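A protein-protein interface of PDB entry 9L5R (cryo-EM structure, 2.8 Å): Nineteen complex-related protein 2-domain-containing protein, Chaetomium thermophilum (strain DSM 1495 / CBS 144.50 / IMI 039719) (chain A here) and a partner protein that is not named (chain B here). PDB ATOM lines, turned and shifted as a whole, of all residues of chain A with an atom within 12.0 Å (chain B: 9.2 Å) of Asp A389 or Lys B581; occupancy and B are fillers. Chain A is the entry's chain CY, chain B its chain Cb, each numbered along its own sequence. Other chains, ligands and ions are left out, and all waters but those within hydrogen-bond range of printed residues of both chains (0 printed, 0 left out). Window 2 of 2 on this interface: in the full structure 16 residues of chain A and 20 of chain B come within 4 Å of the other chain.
Among the printed residues, merely in contact across the chains: Asp A389 with Lys B581, Arg A393 with Ser B583, Pro A392 with Pro B582, Pro A392 with Ala B584 and Arg A393 with Ala B584.
Asp A389 touches one residue of chain B.
Of chain A, only Asp A389 (3.3 Å) comes within 4 Å of Lys B581.
No residue of chain B comes within 4 Å of Pro A388.
Lys B577 touches none of the printed residues of chain A.
No residue of chain A comes within 4 Å of Tyr B579.
Of chain A, only Pro A392 (3.3 Å) comes within 4 Å of Pro B582.
Of the printed residues of chain B, Pro A392 touches Pro B582 and Ala B584.
Printed residues of chain B within 4 Å of Arg A393: Ser B583 (3.3 Å) and Ala B584 (3.9 Å).
Printed residues of chain A within 4 Å of Ala B584: Pro A392 (3.4 Å) and Arg A393 (3.9 Å).
Thr B578 touches none of the printed residues of chain A.
Gly A385 touches none of the printed residues of chain B.
The nearest residue of chain A that does not touch Lys B581 is Asp A390 (5.4 Å).
The nearest printed residue of chain A that does not touch Ala B584 is Met A394 (5.7 Å).
Of the 15 printed residues of chain A, 3 touch a printed residue of chain B.
Of the 10 printed residues of chain B, 4 touch a printed residue of chain A.
Hydrophobic or aromatic side chains of chain B within 4 Å of the printed part of chain A: Ala B584.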
ATOM      1  N   ASP A 381     -33.139 -35.565 -18.546  1.00  0.00           N
ATOM      2  CA  ASP A 381     -31.891 -36.318 -18.581  1.00  0.00           C
ATOM      3  C   ASP A 381     -31.408 -36.512 -20.014  1.00  0.00           C
ATOM      4  O   ASP A 381     -30.222 -36.347 -20.307  1.00  0.00           O
ATOM      5  CB  ASP A 381     -32.062 -37.675 -17.895  1.00  0.00           C
ATOM      6  N   LEU A 382     -32.339 -36.869 -20.902  1.00  0.00           N
ATOM      7  CA  LEU A 382     -31.991 -37.077 -22.304  1.00  0.00           C
ATOM      8  C   LEU A 382     -31.585 -35.772 -22.977  1.00  0.00           C
ATOM      9  O   LEU A 382     -30.702 -35.762 -23.842  1.00  0.00           O
ATOM     10  CB  LEU A 382     -33.163 -37.723 -23.043  1.00  0.00           C
ATOM     11  N   TYR A 383     -32.223 -34.660 -22.594  1.00  0.00           N
ATOM     12  CA  TYR A 383     -31.867 -33.360 -23.156  1.00  0.00           C
ATOM     13  C   TYR A 383     -30.453 -32.948 -22.759  1.00  0.00           C
ATOM     14  O   TYR A 383     -29.688 -32.454 -23.593  1.00  0.00           O
ATOM     15  CB  TYR A 383     -32.879 -32.303 -22.712  1.00  0.00           C
ATOM     16  N   GLU A 384     -30.086 -33.153 -21.491  1.00  0.00           N
ATOM     17  CA  GLU A 384     -28.726 -32.846 -21.060  1.00  0.00           C
ATOM     18  C   GLU A 384     -27.719 -33.834 -21.633  1.00  0.00           C
ATOM     19  O   GLU A 384     -26.555 -33.480 -21.848  1.00  0.00           O
ATOM     20  CB  GLU A 384     -28.649 -32.829 -19.534  1.00  0.00           C
ATOM     21  N   GLY A 385     -28.136 -35.079 -21.869  1.00  0.00           N
ATOM     22  CA  GLY A 385     -27.251 -36.029 -22.519  1.00  0.00           C
ATOM     23  C   GLY A 385     -26.957 -35.668 -23.963  1.00  0.00           C
ATOM     24  O   GLY A 385     -25.806 -35.733 -24.407  1.00  0.00           O
ATOM     25  N   ARG A 386     -27.988 -35.276 -24.714  1.00  0.00           N
ATOM     26  CA  ARG A 386     -27.837 -34.973 -26.130  1.00  0.00           C
ATOM     27  C   ARG A 386     -27.410 -33.537 -26.398  1.00  0.00           C
ATOM     28  O   ARG A 386     -27.053 -33.221 -27.539  1.00  0.00           O
ATOM     29  CB  ARG A 386     -29.148 -35.259 -26.869  1.00  0.00           C
ATOM     30  N   GLY A 387     -27.442 -32.664 -25.395  1.00  0.00           N
ATOM     31  CA  GLY A 387     -27.033 -31.293 -25.573  1.00  0.00           C
ATOM     32  C   GLY A 387     -25.541 -31.179 -25.788  1.00  0.00           C
ATOM     33  O   GLY A 387     -24.741 -31.620 -24.957  1.00  0.00           O
ATOM     34  N   PRO A 388     -25.141 -30.603 -26.929  1.00  0.00           N
ATOM     35  CA  PRO A 388     -23.703 -30.429 -27.204  1.00  0.00           C
ATOM     36  C   PRO A 388     -22.994 -29.545 -26.194  1.00  0.00           C
ATOM     37  O   PRO A 388     -21.812 -29.771 -25.906  1.00  0.00           O
ATOM     38  CB  PRO A 388     -23.691 -29.807 -28.607  1.00  0.00           C
ATOM     39  N   ASP A 389     -23.680 -28.539 -25.651  1.00  0.00           N
ATOM     40  CA  ASP A 389     -23.125 -27.789 -24.530  1.00  0.00           C
ATOM     41  C   ASP A 389     -23.175 -28.610 -23.248  1.00  0.00           C
ATOM     42  O   ASP A 389     -22.222 -28.601 -22.458  1.00  0.00           O
ATOM     43  CB  ASP A 389     -23.878 -26.472 -24.354  1.00  0.00           C
ATOM     44  N   ASP A 390     -24.272 -29.336 -23.029  1.00  0.00           N
ATOM     45  CA  ASP A 390     -24.456 -30.072 -21.786  1.00  0.00           C
ATOM     46  C   ASP A 390     -23.667 -31.377 -21.737  1.00  0.00           C
ATOM     47  O   ASP A 390     -23.348 -31.843 -20.638  1.00  0.00           O
ATOM     48  CB  ASP A 390     -25.942 -30.346 -21.559  1.00  0.00           C
ATOM     49  N   ILE A 391     -23.356 -31.980 -22.882  1.00  0.00           N
ATOM     50  CA  ILE A 391     -22.436 -33.117 -22.908  1.00  0.00           C
ATOM     51  C   ILE A 391     -21.055 -32.566 -22.581  1.00  0.00           C
ATOM     52  O   ILE A 391     -20.461 -31.862 -23.410  1.00  0.00           O
ATOM     53  CB  ILE A 391     -22.449 -33.843 -24.262  1.00  0.00           C
ATOM     54  N   PRO A 392     -20.521 -32.842 -21.395  1.00  0.00           N
ATOM     55  CA  PRO A 392     -19.314 -32.138 -20.952  1.00  0.00           C
ATOM     56  C   PRO A 392     -18.070 -32.565 -21.713  1.00  0.00           C
ATOM     57  O   PRO A 392     -17.962 -33.691 -22.203  1.00  0.00           O
ATOM     58  CB  PRO A 392     -19.210 -32.518 -19.471  1.00  0.00           C
ATOM     59  N   ARG A 393     -17.128 -31.631 -21.819  1.00  0.00           N
ATOM     60  CA  ARG A 393     -15.792 -31.966 -22.282  1.00  0.00           C
ATOM     61  C   ARG A 393     -15.028 -32.666 -21.166  1.00  0.00           C
ATOM     62  O   ARG A 393     -15.109 -32.276 -19.999  1.00  0.00           O
ATOM     63  CB  ARG A 393     -15.050 -30.711 -22.731  1.00  0.00           C
ATOM     64  N   MET A 394     -14.279 -33.700 -21.528  1.00  0.00           N
ATOM     65  CA  MET A 394     -13.650 -34.579 -20.555  1.00  0.00           C
ATOM     66  C   MET A 394     -12.179 -34.232 -20.362  1.00  0.00           C
ATOM     67  O   MET A 394     -11.565 -33.552 -21.188  1.00  0.00           O
ATOM     68  CB  MET A 394     -13.785 -36.042 -20.983  1.00  0.00           C
ATOM     69  N   LYS A 395     -11.630 -34.698 -19.249  1.00  0.00           N
ATOM     70  CA  LYS A 395     -10.225 -34.588 -18.893  1.00  0.00           C
ATOM     71  C   LYS A 395      -9.800 -35.864 -18.187  1.00  0.00           C
ATOM     72  O   LYS A 395     -10.642 -36.603 -17.664  1.00  0.00           O
ATOM     73  CB  LYS A 395      -9.966 -33.374 -17.988  1.00  0.00           C
ATOM     74  N   LYS B 575     -23.232 -28.350 -11.148  1.00  0.00           N
ATOM     75  CA  LYS B 575     -22.895 -26.930 -11.067  1.00  0.00           C
ATOM     76  C   LYS B 575     -22.863 -26.370 -12.484  1.00  0.00           C
ATOM     77  O   LYS B 575     -21.901 -26.582 -13.226  1.00  0.00           O
ATOM     78  CB  LYS B 575     -21.563 -26.731 -10.350  1.00  0.00           C
ATOM     79  N   LYS B 576     -23.916 -25.650 -12.859  1.00  0.00           N
ATOM     80  CA  LYS B 576     -24.059 -25.121 -14.210  1.00  0.00           C
ATOM     81  C   LYS B 576     -23.714 -23.637 -14.215  1.00  0.00           C
ATOM     82  O   LYS B 576     -24.275 -22.861 -13.434  1.00  0.00           O
ATOM     83  CB  LYS B 576     -25.478 -25.347 -14.728  1.00  0.00           C
ATOM     84  N   LYS B 577     -22.796 -23.247 -15.095  1.00  0.00           N
ATOM     85  CA  LYS B 577     -22.359 -21.864 -15.186  1.00  0.00           C
ATOM     86  C   LYS B 577     -23.313 -21.045 -16.053  1.00  0.00           C
ATOM     87  O   LYS B 577     -24.350 -21.529 -16.516  1.00  0.00           O
ATOM     88  CB  LYS B 577     -20.941 -21.784 -15.748  1.00  0.00           C
ATOM     89  N   THR B 578     -22.950 -19.777 -16.254  1.00  0.00           N
ATOM     90  CA  THR B 578     -23.771 -18.883 -17.065  1.00  0.00           C
ATOM     91  C   THR B 578     -23.315 -18.852 -18.520  1.00  0.00           C
ATOM     92  O   THR B 578     -24.132 -18.637 -19.423  1.00  0.00           O
ATOM     93  CB  THR B 578     -23.750 -17.472 -16.475  1.00  0.00           C
ATOM     94  N   TYR B 579     -22.025 -19.054 -18.769  1.00  0.00           N
ATOM     95  CA  TYR B 579     -21.474 -18.955 -20.117  1.00  0.00           C
ATOM     96  C   TYR B 579     -20.672 -20.174 -20.545  1.00  0.00           C
ATOM     97  O   TYR B 579     -20.717 -20.550 -21.720  1.00  0.00           O
ATOM     98  CB  TYR B 579     -20.591 -17.704 -20.230  1.00  0.00           C
ATOM     99  N   ARG B 580     -19.940 -20.808 -19.632  1.00  0.00           N
ATOM    100  CA  ARG B 580     -19.038 -21.898 -19.975  1.00  0.00           C
ATOM    101  C   ARG B 580     -19.648 -23.245 -19.604  1.00  0.00           C
ATOM    102  O   ARG B 580     -20.263 -23.392 -18.545  1.00  0.00           O
ATOM    103  CB  ARG B 580     -17.690 -21.726 -19.270  1.00  0.00           C
ATOM    104  N   LYS B 581     -19.475 -24.221 -20.487  1.00  0.00           N
ATOM    105  CA  LYS B 581     -19.976 -25.564 -20.223  1.00  0.00           C
ATOM    106  C   LYS B 581     -19.141 -26.224 -19.130  1.00  0.00           C
ATOM    107  O   LYS B 581     -17.907 -26.234 -19.219  1.00  0.00           O
ATOM    108  CB  LYS B 581     -19.940 -26.407 -21.496  1.00  0.00           C
ATOM    109  N   PRO B 582     -19.765 -26.780 -18.092  1.00  0.00           N
ATOM    110  CA  PRO B 582     -18.982 -27.365 -16.996  1.00  0.00           C
ATOM    111  C   PRO B 582     -18.429 -28.728 -17.384  1.00  0.00           C
ATOM    112  O   PRO B 582     -19.172 -29.621 -17.799  1.00  0.00           O
ATOM    113  CB  PRO B 582     -19.995 -27.471 -15.852  1.00  0.00           C
ATOM    114  N   SER B 583     -17.114 -28.877 -17.257  1.00  0.00           N
ATOM    115  CA  SER B 583     -16.490 -30.177 -17.453  1.00  0.00           C
ATOM    116  C   SER B 583     -16.884 -31.114 -16.319  1.00  0.00           C
ATOM    117  O   SER B 583     -16.905 -30.723 -15.149  1.00  0.00           O
ATOM    118  CB  SER B 583     -14.970 -30.035 -17.520  1.00  0.00           C
ATOM    119  N   ALA B 584     -17.201 -32.356 -16.672  1.00  0.00           N
ATOM    120  CA  ALA B 584     -17.742 -33.298 -15.704  1.00  0.00           C
ATOM    121  C   ALA B 584     -16.670 -33.750 -14.717  1.00  0.00           C
ATOM    122  O   ALA B 584     -15.489 -33.408 -14.834  1.00  0.00           O
ATOM    123  CB  ALA B 584     -18.341 -34.511 -16.413  1.00  0.00           C
